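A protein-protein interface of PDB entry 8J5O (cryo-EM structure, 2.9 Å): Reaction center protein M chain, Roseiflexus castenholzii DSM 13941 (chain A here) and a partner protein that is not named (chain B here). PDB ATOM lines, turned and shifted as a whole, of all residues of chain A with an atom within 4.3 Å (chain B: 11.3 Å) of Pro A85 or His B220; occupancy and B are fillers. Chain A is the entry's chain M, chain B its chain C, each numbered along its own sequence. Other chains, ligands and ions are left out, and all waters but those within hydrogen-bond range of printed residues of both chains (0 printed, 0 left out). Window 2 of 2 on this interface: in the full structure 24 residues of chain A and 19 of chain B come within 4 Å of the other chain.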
ATOM      1  N   VAL A  83     -12.440 -17.425   8.176  1.00  0.00           N
ATOM      2  CA  VAL A  83     -12.652 -18.379   9.262  1.00  0.00           C
ATOM      3  C   VAL A  83     -13.818 -17.838  10.081  1.00  0.00           C
ATOM      4  O   VAL A  83     -13.640 -17.015  10.980  1.00  0.00           O
ATOM      5  CB  VAL A  83     -11.400 -18.570  10.122  1.00  0.00           C
ATOM      6  CG1 VAL A  83     -11.727 -19.365  11.371  1.00  0.00           C
ATOM      7  CG2 VAL A  83     -10.307 -19.255   9.320  1.00  0.00           C
ATOM      8  N   TYR A  84     -15.025 -18.299   9.775  1.00  0.00           N
ATOM      9  CA  TYR A  84     -16.231 -17.728  10.352  1.00  0.00           C
ATOM     10  C   TYR A  84     -16.489 -18.251  11.761  1.00  0.00           C
ATOM     11  O   TYR A  84     -15.991 -19.310  12.146  1.00  0.00           O
ATOM     12  CB  TYR A  84     -17.429 -18.029   9.461  1.00  0.00           C
ATOM     13  CG  TYR A  84     -17.276 -17.510   8.054  1.00  0.00           C
ATOM     14  CD1 TYR A  84     -17.445 -16.163   7.769  1.00  0.00           C
ATOM     15  CD2 TYR A  84     -16.952 -18.365   7.011  1.00  0.00           C
ATOM     16  CE1 TYR A  84     -17.303 -15.684   6.486  1.00  0.00           C
ATOM     17  CE2 TYR A  84     -16.808 -17.895   5.725  1.00  0.00           C
ATOM     18  CZ  TYR A  84     -16.983 -16.555   5.467  1.00  0.00           C
ATOM     19  OH  TYR A  84     -16.838 -16.085   4.185  1.00  0.00           O
ATOM     20  N   PRO A  85     -17.271 -17.520  12.550  1.00  0.00           N
ATOM     21  CA  PRO A  85     -17.646 -17.996  13.883  1.00  0.00           C
ATOM     22  C   PRO A  85     -18.657 -19.124  13.795  1.00  0.00           C
ATOM     23  O   PRO A  85     -19.106 -19.483  12.697  1.00  0.00           O
ATOM     24  CB  PRO A  85     -18.253 -16.750  14.544  1.00  0.00           C
ATOM     25  CG  PRO A  85     -18.701 -15.906  13.417  1.00  0.00           C
ATOM     26  CD  PRO A  85     -17.748 -16.151  12.294  1.00  0.00           C
ATOM     27  N   PRO A  86     -19.026 -19.719  14.928  1.00  0.00           N
ATOM     28  CA  PRO A  86     -19.978 -20.823  14.894  1.00  0.00           C
ATOM     29  C   PRO A  86     -21.336 -20.351  14.399  1.00  0.00           C
ATOM     30  O   PRO A  86     -21.697 -19.172  14.563  1.00  0.00           O
ATOM     31  CB  PRO A  86     -20.042 -21.281  16.356  1.00  0.00           C
ATOM     32  CG  PRO A  86     -18.743 -20.850  16.935  1.00  0.00           C
ATOM     33  CD  PRO A  86     -18.429 -19.550  16.264  1.00  0.00           C
ATOM     34  N   PRO A  87     -22.110 -21.240  13.781  1.00  0.00           N
ATOM     35  CA  PRO A  87     -23.434 -20.855  13.275  1.00  0.00           C
ATOM     36  C   PRO A  87     -24.376 -20.436  14.395  1.00  0.00           C
ATOM     37  O   PRO A  87     -24.060 -20.511  15.585  1.00  0.00           O
ATOM     38  CB  PRO A  87     -23.926 -22.126  12.575  1.00  0.00           C
ATOM     39  CG  PRO A  87     -22.681 -22.858  12.220  1.00  0.00           C
ATOM     40  CD  PRO A  87     -21.725 -22.589  13.339  1.00  0.00           C
ATOM     41  N   THR A  88     -25.569 -19.989  13.987  1.00  0.00           N
ATOM     42  CA  THR A  88     -26.509 -19.394  14.934  1.00  0.00           C
ATOM     43  C   THR A  88     -27.006 -20.404  15.961  1.00  0.00           C
ATOM     44  O   THR A  88     -27.267 -20.036  17.111  1.00  0.00           O
ATOM     45  CB  THR A  88     -27.690 -18.774  14.189  1.00  0.00           C
ATOM     46  OG1 THR A  88     -27.205 -17.841  13.217  1.00  0.00           O
ATOM     47  CG2 THR A  88     -28.601 -18.044  15.159  1.00  0.00           C
ATOM     48  N   GLY A 101     -16.189 -23.327  13.527  1.00  0.00           N
ATOM     49  CA  GLY A 101     -16.047 -22.220  14.451  1.00  0.00           C
ATOM     50  C   GLY A 101     -15.095 -22.453  15.602  1.00  0.00           C
ATOM     51  O   GLY A 101     -14.921 -21.548  16.424  1.00  0.00           O
ATOM     52  N   TRP A 104     -11.969 -20.032  15.236  1.00  0.00           N
ATOM     53  CA  TRP A 104     -12.285 -18.618  15.398  1.00  0.00           C
ATOM     54  C   TRP A 104     -12.187 -18.189  16.856  1.00  0.00           C
ATOM     55  O   TRP A 104     -11.646 -17.119  17.160  1.00  0.00           O
ATOM     56  CB  TRP A 104     -13.681 -18.338  14.836  1.00  0.00           C
ATOM     57  CG  TRP A 104     -14.066 -16.892  14.816  1.00  0.00           C
ATOM     58  CD1 TRP A 104     -13.916 -16.018  13.783  1.00  0.00           C
ATOM     59  CD2 TRP A 104     -14.709 -16.164  15.866  1.00  0.00           C
ATOM     60  NE1 TRP A 104     -14.401 -14.784  14.132  1.00  0.00           N
ATOM     61  CE2 TRP A 104     -14.896 -14.847  15.407  1.00  0.00           C
ATOM     62  CE3 TRP A 104     -15.136 -16.494  17.155  1.00  0.00           C
ATOM     63  CZ2 TRP A 104     -15.490 -13.862  16.189  1.00  0.00           C
ATOM     64  CZ3 TRP A 104     -15.724 -15.516  17.929  1.00  0.00           C
ATOM     65  CH2 TRP A 104     -15.895 -14.216  17.445  1.00  0.00           C
ATOM     66  N   TRP A 160     -22.519 -16.316  18.695  1.00  0.00           N
ATOM     67  CA  TRP A 160     -21.226 -15.871  18.196  1.00  0.00           C
ATOM     68  C   TRP A 160     -21.281 -15.396  16.753  1.00  0.00           C
ATOM     69  O   TRP A 160     -20.322 -14.775  16.286  1.00  0.00           O
ATOM     70  CB  TRP A 160     -20.197 -17.000  18.306  1.00  0.00           C
ATOM     71  CG  TRP A 160     -19.654 -17.221  19.682  1.00  0.00           C
ATOM     72  CD1 TRP A 160     -19.714 -18.371  20.407  1.00  0.00           C
ATOM     73  CD2 TRP A 160     -18.957 -16.269  20.494  1.00  0.00           C
ATOM     74  NE1 TRP A 160     -19.102 -18.197  21.622  1.00  0.00           N
ATOM     75  CE2 TRP A 160     -18.629 -16.915  21.700  1.00  0.00           C
ATOM     76  CE3 TRP A 160     -18.580 -14.935  20.319  1.00  0.00           C
ATOM     77  CZ2 TRP A 160     -17.944 -16.272  22.727  1.00  0.00           C
ATOM     78  CZ3 TRP A 160     -17.900 -14.299  21.340  1.00  0.00           C
ATOM     79  CH2 TRP A 160     -17.587 -14.968  22.527  1.00  0.00           C
ATOM     80  N   SER A 161     -22.376 -15.667  16.040  1.00  0.00           N
ATOM     81  CA  SER A 161     -22.478 -15.336  14.625  1.00  0.00           C
ATOM     82  C   SER A 161     -22.596 -13.842  14.366  1.00  0.00           C
ATOM     83  O   SER A 161     -22.529 -13.428  13.206  1.00  0.00           O
ATOM     84  CB  SER A 161     -23.673 -16.059  14.006  1.00  0.00           C
ATOM     85  OG  SER A 161     -23.533 -17.459  14.129  1.00  0.00           O
ATOM     86  N   ALA A 163     -20.442 -11.645  14.895  1.00  0.00           N
ATOM     87  CA  ALA A 163     -19.086 -11.127  14.843  1.00  0.00           C
ATOM     88  C   ALA A 163     -18.452 -11.414  13.487  1.00  0.00           C
ATOM     89  O   ALA A 163     -18.872 -12.336  12.777  1.00  0.00           O
ATOM     90  CB  ALA A 163     -18.226 -11.742  15.956  1.00  0.00           C
ATOM     91  N   PRO A 164     -17.444 -10.635  13.093  1.00  0.00           N
ATOM     92  CA  PRO A 164     -16.828 -10.828  11.776  1.00  0.00           C
ATOM     93  C   PRO A 164     -16.065 -12.142  11.682  1.00  0.00           C
ATOM     94  O   PRO A 164     -15.715 -12.769  12.683  1.00  0.00           O
ATOM     95  CB  PRO A 164     -15.886  -9.628  11.650  1.00  0.00           C
ATOM     96  CG  PRO A 164     -16.471  -8.601  12.550  1.00  0.00           C
ATOM     97  CD  PRO A 164     -17.030  -9.364  13.709  1.00  0.00           C
ATOM     98  N   GLY A 165     -15.797 -12.550  10.442  1.00  0.00           N
ATOM     99  CA  GLY A 165     -15.246 -13.864  10.171  1.00  0.00           C
ATOM    100  C   GLY A 165     -13.766 -13.966   9.853  1.00  0.00           C
ATOM    101  O   GLY A 165     -13.334 -14.988   9.316  1.00  0.00           O
ATOM    102  N   PRO B 194     -20.757 -19.337  -3.889  1.00  0.00           N
ATOM    103  CA  PRO B 194     -20.119 -20.655  -3.807  1.00  0.00           C
ATOM    104  C   PRO B 194     -20.587 -21.549  -4.944  1.00  0.00           C
ATOM    105  O   PRO B 194     -21.732 -21.464  -5.392  1.00  0.00           O
ATOM    106  CB  PRO B 194     -20.574 -21.188  -2.445  1.00  0.00           C
ATOM    107  CG  PRO B 194     -20.926 -19.974  -1.661  1.00  0.00           C
ATOM    108  CD  PRO B 194     -21.479 -18.996  -2.653  1.00  0.00           C
ATOM    109  N   TRP B 197     -23.959 -23.747  -4.596  1.00  0.00           N
ATOM    110  CA  TRP B 197     -25.171 -23.133  -4.076  1.00  0.00           C
ATOM    111  C   TRP B 197     -26.348 -23.403  -5.004  1.00  0.00           C
ATOM    112  O   TRP B 197     -26.209 -23.390  -6.230  1.00  0.00           O
ATOM    113  CB  TRP B 197     -24.970 -21.625  -3.894  1.00  0.00           C
ATOM    114  CG  TRP B 197     -26.227 -20.876  -3.553  1.00  0.00           C
ATOM    115  CD1 TRP B 197     -26.717 -20.627  -2.306  1.00  0.00           C
ATOM    116  CD2 TRP B 197     -27.147 -20.270  -4.472  1.00  0.00           C
ATOM    117  NE1 TRP B 197     -27.887 -19.915  -2.390  1.00  0.00           N
ATOM    118  CE2 TRP B 197     -28.174 -19.684  -3.708  1.00  0.00           C
ATOM    119  CE3 TRP B 197     -27.208 -20.179  -5.865  1.00  0.00           C
ATOM    120  CZ2 TRP B 197     -29.242 -19.011  -4.290  1.00  0.00           C
ATOM    121  CZ3 TRP B 197     -28.271 -19.512  -6.439  1.00  0.00           C
ATOM    122  CH2 TRP B 197     -29.272 -18.936  -5.654  1.00  0.00           C
ATOM    123  N   PRO B 200     -33.118 -22.186  -2.471  1.00  0.00           N
ATOM    124  CA  PRO B 200     -33.775 -22.899  -1.354  1.00  0.00           C
ATOM    125  C   PRO B 200     -35.269 -23.106  -1.586  1.00  0.00           C
ATOM    126  O   PRO B 200     -36.133 -22.382  -1.093  1.00  0.00           O
ATOM    127  CB  PRO B 200     -33.497 -21.981  -0.161  1.00  0.00           C
ATOM    128  CG  PRO B 200     -33.269 -20.612  -0.749  1.00  0.00           C
ATOM    129  CD  PRO B 200     -33.042 -20.735  -2.231  1.00  0.00           C
ATOM    130  N   LEU B 203     -38.977 -23.774   1.130  1.00  0.00           N
ATOM    131  CA  LEU B 203     -39.474 -22.775   2.060  1.00  0.00           C
ATOM    132  C   LEU B 203     -40.746 -22.136   1.515  1.00  0.00           C
ATOM    133  O   LEU B 203     -41.120 -22.333   0.357  1.00  0.00           O
ATOM    134  CB  LEU B 203     -38.415 -21.695   2.319  1.00  0.00           C
ATOM    135  CG  LEU B 203     -37.139 -22.141   3.038  1.00  0.00           C
ATOM    136  CD1 LEU B 203     -36.135 -21.003   3.095  1.00  0.00           C
ATOM    137  CD2 LEU B 203     -37.446 -22.655   4.437  1.00  0.00           C
ATOM    138  N   GLY B 208     -40.416 -16.616   3.396  1.00  0.00           N
ATOM    139  CA  GLY B 208     -39.274 -17.516   3.470  1.00  0.00           C
ATOM    140  C   GLY B 208     -37.951 -16.823   3.747  1.00  0.00           C
ATOM    141  O   GLY B 208     -37.145 -17.309   4.546  1.00  0.00           O
ATOM    142  N   LEU B 209     -37.700 -15.693   3.089  1.00  0.00           N
ATOM    143  CA  LEU B 209     -36.403 -15.022   3.128  1.00  0.00           C
ATOM    144  C   LEU B 209     -36.456 -13.693   3.878  1.00  0.00           C
ATOM    145  O   LEU B 209     -35.839 -12.711   3.468  1.00  0.00           O
ATOM    146  CB  LEU B 209     -35.866 -14.804   1.716  1.00  0.00           C
ATOM    147  CG  LEU B 209     -35.569 -16.035   0.857  1.00  0.00           C
ATOM    148  CD1 LEU B 209     -35.769 -15.711  -0.614  1.00  0.00           C
ATOM    149  CD2 LEU B 209     -34.159 -16.542   1.102  1.00  0.00           C
ATOM    150  N   VAL B 210     -37.190 -13.646   4.983  1.00  0.00           N
ATOM    151  CA  VAL B 210     -37.305 -12.439   5.793  1.00  0.00           C
ATOM    152  C   VAL B 210     -36.261 -12.483   6.902  1.00  0.00           C
ATOM    153  O   VAL B 210     -36.127 -13.496   7.597  1.00  0.00           O
ATOM    154  CB  VAL B 210     -38.722 -12.303   6.371  1.00  0.00           C
ATOM    155  CG1 VAL B 210     -38.797 -11.123   7.321  1.00  0.00           C
ATOM    156  CG2 VAL B 210     -39.731 -12.149   5.248  1.00  0.00           C
ATOM    157  N   VAL B 211     -35.511 -11.392   7.062  1.00  0.00           N
ATOM    158  CA  VAL B 211     -34.433 -11.352   8.044  1.00  0.00           C
ATOM    159  C   VAL B 211     -34.481 -10.084   8.891  1.00  0.00           C
ATOM    160  O   VAL B 211     -33.822 -10.002   9.932  1.00  0.00           O
ATOM    161  CB  VAL B 211     -33.058 -11.478   7.358  1.00  0.00           C
ATOM    162  CG1 VAL B 211     -32.937 -12.807   6.637  1.00  0.00           C
ATOM    163  CG2 VAL B 211     -32.831 -10.315   6.402  1.00  0.00           C
ATOM    164  N   ARG B 214     -35.645  -9.858  12.834  1.00  0.00           N
ATOM    165  CA  ARG B 214     -36.250 -11.098  13.311  1.00  0.00           C
ATOM    166  C   ARG B 214     -35.769 -11.451  14.711  1.00  0.00           C
ATOM    167  O   ARG B 214     -36.562 -11.883  15.557  1.00  0.00           O
ATOM    168  CB  ARG B 214     -35.948 -12.234  12.337  1.00  0.00           C
ATOM    169  CG  ARG B 214     -36.665 -12.113  11.005  1.00  0.00           C
ATOM    170  CD  ARG B 214     -37.900 -12.990  10.960  1.00  0.00           C
ATOM    171  NE  ARG B 214     -37.606 -14.364  11.343  1.00  0.00           N
ATOM    172  CZ  ARG B 214     -37.188 -15.303  10.506  1.00  0.00           C
ATOM    173  NH1 ARG B 214     -36.995 -15.049   9.223  1.00  0.00           N
ATOM    174  NH2 ARG B 214     -36.956 -16.527  10.968  1.00  0.00           N
ATOM    175  N   LYS B 215     -34.465 -11.312  14.960  1.00  0.00           N
ATOM    176  CA  LYS B 215     -33.857 -11.489  16.277  1.00  0.00           C
ATOM    177  C   LYS B 215     -33.775 -12.964  16.674  1.00  0.00           C
ATOM    178  O   LYS B 215     -33.177 -13.304  17.700  1.00  0.00           O
ATOM    179  CB  LYS B 215     -34.618 -10.668  17.325  1.00  0.00           C
ATOM    180  CG  LYS B 215     -34.046 -10.715  18.730  1.00  0.00           C
ATOM    181  CD  LYS B 215     -34.800  -9.783  19.660  1.00  0.00           C
ATOM    182  CE  LYS B 215     -34.329  -9.935  21.095  1.00  0.00           C
ATOM    183  NZ  LYS B 215     -32.917  -9.490  21.264  1.00  0.00           N
ATOM    184  N   ASP B 216     -34.351 -13.850  15.864  1.00  0.00           N
ATOM    185  CA  ASP B 216     -34.138 -15.285  15.991  1.00  0.00           C
ATOM    186  C   ASP B 216     -33.190 -15.830  14.932  1.00  0.00           C
ATOM    187  O   ASP B 216     -32.958 -17.042  14.889  1.00  0.00           O
ATOM    188  CB  ASP B 216     -35.480 -16.033  15.942  1.00  0.00           C
ATOM    189  CG  ASP B 216     -36.216 -15.859  14.618  1.00  0.00           C
ATOM    190  OD1 ASP B 216     -35.731 -15.126  13.733  1.00  0.00           O
ATOM    191  OD2 ASP B 216     -37.291 -16.473  14.461  1.00  0.00           O
ATOM    192  N   VAL B 217     -32.639 -14.964  14.083  1.00  0.00           N
ATOM    193  CA  VAL B 217     -31.670 -15.359  13.067  1.00  0.00           C
ATOM    194  C   VAL B 217     -30.400 -14.552  13.283  1.00  0.00           C
ATOM    195  O   VAL B 217     -30.332 -13.715  14.188  1.00  0.00           O
ATOM    196  CB  VAL B 217     -32.228 -15.155  11.646  1.00  0.00           C
ATOM    197  CG1 VAL B 217     -33.456 -16.020  11.431  1.00  0.00           C
ATOM    198  CG2 VAL B 217     -32.550 -13.689  11.404  1.00  0.00           C
ATOM    199  N   SER B 218     -29.388 -14.791  12.457  1.00  0.00           N
ATOM    200  CA  SER B 218     -28.118 -14.091  12.595  1.00  0.00           C
ATOM    201  C   SER B 218     -27.500 -13.960  11.205  1.00  0.00           C
ATOM    202  O   SER B 218     -28.193 -14.088  10.192  1.00  0.00           O
ATOM    203  CB  SER B 218     -27.214 -14.815  13.606  1.00  0.00           C
ATOM    204  OG  SER B 218     -25.966 -14.162  13.728  1.00  0.00           O
ATOM    205  N   ASN B 219     -26.193 -13.694  11.156  1.00  0.00           N
ATOM    206  CA  ASN B 219     -25.536 -13.354   9.898  1.00  0.00           C
ATOM    207  C   ASN B 219     -25.556 -14.488   8.878  1.00  0.00           C
ATOM    208  O   ASN B 219     -25.423 -14.222   7.680  1.00  0.00           O
ATOM    209  CB  ASN B 219     -24.095 -12.918  10.164  1.00  0.00           C
ATOM    210  CG  ASN B 219     -24.012 -11.560  10.835  1.00  0.00           C
ATOM    211  OD1 ASN B 219     -24.982 -10.807  10.860  1.00  0.00           O
ATOM    212  ND2 ASN B 219     -22.846 -11.242  11.381  1.00  0.00           N
ATOM    213  N   HIS B 220     -25.710 -15.743   9.309  1.00  0.00           N
ATOM    214  CA  HIS B 220     -25.749 -16.846   8.350  1.00  0.00           C
ATOM    215  C   HIS B 220     -27.018 -16.802   7.501  1.00  0.00           C
ATOM    216  O   HIS B 220     -26.967 -16.996   6.276  1.00  0.00           O
ATOM    217  CB  HIS B 220     -25.637 -18.181   9.084  1.00  0.00           C
ATOM    218  CG  HIS B 220     -24.228 -18.609   9.348  1.00  0.00           C
ATOM    219  ND1 HIS B 220     -23.684 -18.643  10.614  1.00  0.00           N
ATOM    220  CD2 HIS B 220     -23.249 -19.024   8.508  1.00  0.00           C
ATOM    221  CE1 HIS B 220     -22.431 -19.056  10.543  1.00  0.00           C
ATOM    222  NE2 HIS B 220     -22.143 -19.296   9.276  1.00  0.00           N
ATOM    223  N   GLU B 221     -28.165 -16.545   8.131  1.00  0.00           N
ATOM    224  CA  GLU B 221     -29.409 -16.412   7.381  1.00  0.00           C
ATOM    225  C   GLU B 221     -29.357 -15.209   6.449  1.00  0.00           C
ATOM    226  O   GLU B 221     -29.871 -15.260   5.324  1.00  0.00           O
ATOM    227  CB  GLU B 221     -30.592 -16.300   8.342  1.00  0.00           C
ATOM    228  CG  GLU B 221     -30.916 -17.577   9.106  1.00  0.00           C
ATOM    229  CD  GLU B 221     -30.006 -17.795  10.301  1.00  0.00           C
ATOM    230  OE1 GLU B 221     -28.981 -17.091  10.402  1.00  0.00           O
ATOM    231  OE2 GLU B 221     -30.315 -18.666  11.141  1.00  0.00           O
ATOM    232  N   VAL B 222     -28.736 -14.117   6.898  1.00  0.00           N
ATOM    233  CA  VAL B 222     -28.577 -12.946   6.043  1.00  0.00           C
ATOM    234  C   VAL B 222     -27.689 -13.277   4.850  1.00  0.00           C
ATOM    235  O   VAL B 222     -27.921 -12.801   3.734  1.00  0.00           O
ATOM    236  CB  VAL B 222     -28.022 -11.761   6.854  1.00  0.00           C
ATOM    237  CG1 VAL B 222     -27.760 -10.578   5.942  1.00  0.00           C
ATOM    238  CG2 VAL B 222     -28.981 -11.380   7.967  1.00  0.00           C
ATOM    239  N   GLU B 223     -26.658 -14.097   5.065  1.00  0.00           N
ATOM    240  CA  GLU B 223     -25.797 -14.512   3.962  1.00  0.00           C
ATOM    241  C   GLU B 223     -26.563 -15.343   2.941  1.00  0.00           C
ATOM    242  O   GLU B 223     -26.392 -15.166   1.728  1.00  0.00           O
ATOM    243  CB  GLU B 223     -24.604 -15.296   4.504  1.00  0.00           C
ATOM    244  CG  GLU B 223     -23.488 -15.498   3.501  1.00  0.00           C
ATOM    245  CD  GLU B 223     -22.343 -16.310   4.064  1.00  0.00           C
ATOM    246  OE1 GLU B 223     -22.610 -17.264   4.826  1.00  0.00           O
ATOM    247  OE2 GLU B 223     -21.176 -15.994   3.748  1.00  0.00           O
ATOM    248  N   GLN B 224     -27.403 -16.267   3.413  1.00  0.00           N
ATOM    249  CA  GLN B 224     -28.215 -17.060   2.491  1.00  0.00           C
ATOM    250  C   GLN B 224     -29.180 -16.177   1.705  1.00  0.00           C
ATOM    251  O   GLN B 224     -29.353 -16.348   0.485  1.00  0.00           O
ATOM    252  CB  GLN B 224     -28.975 -18.137   3.264  1.00  0.00           C
ATOM    253  CG  GLN B 224     -28.078 -19.136   3.971  1.00  0.00           C
ATOM    254  CD  GLN B 224     -27.439 -20.127   3.019  1.00  0.00           C
ATOM    255  OE1 GLN B 224     -26.216 -20.241   2.952  1.00  0.00           O
ATOM    256  NE2 GLN B 224     -28.267 -20.854   2.280  1.00  0.00           N
ATOM    257  N   ASN B 225     -29.809 -15.220   2.391  1.00  0.00           N
ATOM    258  CA  ASN B 225     -30.683 -14.261   1.726  1.00  0.00           C
ATOM    259  C   ASN B 225     -29.927 -13.481   0.659  1.00  0.00           C
ATOM    260  O   ASN B 225     -30.444 -13.254  -0.440  1.00  0.00           O
ATOM    261  CB  ASN B 225     -31.294 -13.323   2.771  1.00  0.00           C
ATOM    262  CG  ASN B 225     -32.084 -12.180   2.158  1.00  0.00           C
ATOM    263  OD1 ASN B 225     -33.290 -12.290   1.954  1.00  0.00           O
ATOM    264  ND2 ASN B 225     -31.415 -11.064   1.899  1.00  0.00           N
ATOM    265  N   GLN B 226     -28.695 -13.068   0.964  1.00  0.00           N
ATOM    266  CA  GLN B 226     -27.900 -12.306   0.007  1.00  0.00           C
ATOM    267  C   GLN B 226     -27.520 -13.149  -1.203  1.00  0.00           C
ATOM    268  O   GLN B 226     -27.487 -12.641  -2.330  1.00  0.00           O
ATOM    269  CB  GLN B 226     -26.655 -11.749   0.691  1.00  0.00           C
ATOM    270  CG  GLN B 226     -26.948 -10.615   1.648  1.00  0.00           C
ATOM    271  CD  GLN B 226     -27.790  -9.528   1.017  1.00  0.00           C
ATOM    272  OE1 GLN B 226     -28.982  -9.414   1.288  1.00  0.00           O
ATOM    273  NE2 GLN B 226     -27.169  -8.718   0.172  1.00  0.00           N
ATOM    274  N   PHE B 227     -27.215 -14.432  -0.994  1.00  0.00           N
ATOM    275  CA  PHE B 227     -26.939 -15.313  -2.127  1.00  0.00           C
ATOM    276  C   PHE B 227     -28.148 -15.403  -3.051  1.00  0.00           C
ATOM    277  O   PHE B 227     -28.026 -15.266  -4.279  1.00  0.00           O
ATOM    278  CB  PHE B 227     -26.542 -16.708  -1.642  1.00  0.00           C
ATOM    279  CG  PHE B 227     -25.196 -16.768  -0.985  1.00  0.00           C
ATOM    280  CD1 PHE B 227     -24.163 -15.951  -1.407  1.00  0.00           C
ATOM    281  CD2 PHE B 227     -24.957 -17.664   0.043  1.00  0.00           C
ATOM    282  CE1 PHE B 227     -22.925 -16.012  -0.804  1.00  0.00           C
ATOM    283  CE2 PHE B 227     -23.720 -17.731   0.647  1.00  0.00           C
ATOM    284  CZ  PHE B 227     -22.703 -16.904   0.223  1.00  0.00           C
ATOM    285  N   ALA B 228     -29.334 -15.612  -2.472  1.00  0.00           N
ATOM    286  CA  ALA B 228     -30.543 -15.686  -3.291  1.00  0.00           C
ATOM    287  C   ALA B 228     -30.802 -14.374  -4.026  1.00  0.00           C
ATOM    288  O   ALA B 228     -31.171 -14.372  -5.209  1.00  0.00           O
ATOM    289  CB  ALA B 228     -31.743 -16.057  -2.420  1.00  0.00           C
ATOM    290  N   MET B 229     -30.604 -13.247  -3.344  1.00  0.00           N
ATOM    291  CA  MET B 229     -30.873 -11.949  -3.953  1.00  0.00           C
ATOM    292  C   MET B 229     -29.909 -11.653  -5.096  1.00  0.00           C
ATOM    293  O   MET B 229     -30.316 -11.122  -6.136  1.00  0.00           O
ATOM    294  CB  MET B 229     -30.809 -10.858  -2.889  1.00  0.00           C
ATOM    295  CG  MET B 229     -31.932 -10.926  -1.870  1.00  0.00           C
ATOM    296  SD  MET B 229     -33.568 -10.628  -2.568  1.00  0.00           S
ATOM    297  CE  MET B 229     -34.407 -12.121  -2.060  1.00  0.00           C
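Printed residues of chain B within 4 Å of Pro A85: His B220.
No residue of chain B comes within 4 Å of Pro A86.
Ser A161 touches three residues of chain B.
No residue of chain B comes within 4 Å of Ala A163.
Of the printed residues of chain A, Ser B218 touches Thr A88 (3.1 Å) and Ser A161 (3.0 Å).
Printed residues of chain A within 4 Å of Asn B219: Ser A161 (2.9 Å).
Of the printed residues of chain A, His B220 touches Pro A85, Pro A87 and Ser A161.
The nearest printed residue of chain A that does not touch His B220 is Pro A86 (4.1 Å).
The backbone NH (N) of Ser B218 sits at hydrogen-bond distance from the side-chain carboxylate (OE1) of Glu B221, 3.1 Å away.
The backbone carbonyl oxygen (O) of Pro A86 lies within hydrogen-bond range of the side-chain hydroxyl (OG) of Ser A161 (2.5 Å).
OG of Ser A161 lies close to O of Pro A87 (3.4 Å).
The side-chain hydroxyl (OG) of Ser A161 lies within hydrogen-bond range of the backbone NH (N) of Thr A88 (3.3 Å).
Hydrophobic or aromatic side chains of chain B within 4 Å of the printed part of chain A: His B220.
Of the 13 printed residues of chain A, 4 touch a printed residue of chain B.
Printed residues of chain A that touch a printed residue of chain B: Pro A85, Pro A87, Thr A88 and Ser A161.
The side-chain amide nitrogen (ND2) of Asn B219 is in hydrogen-bond range of the backbone carbonyl oxygen (O) of Ser A161.
The side-chain carboxylate of Glu B221 is in hydrogen-bond range of the side-chain hydroxyl of Thr A88 (3.4 Å).
Among the printed residues, merely in contact across the chains: Pro A85 with His B220, Pro A87 with His B220, Thr A88 with Ser B218, Ser A161 with Ser B218 and Ser A161 with His B220.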
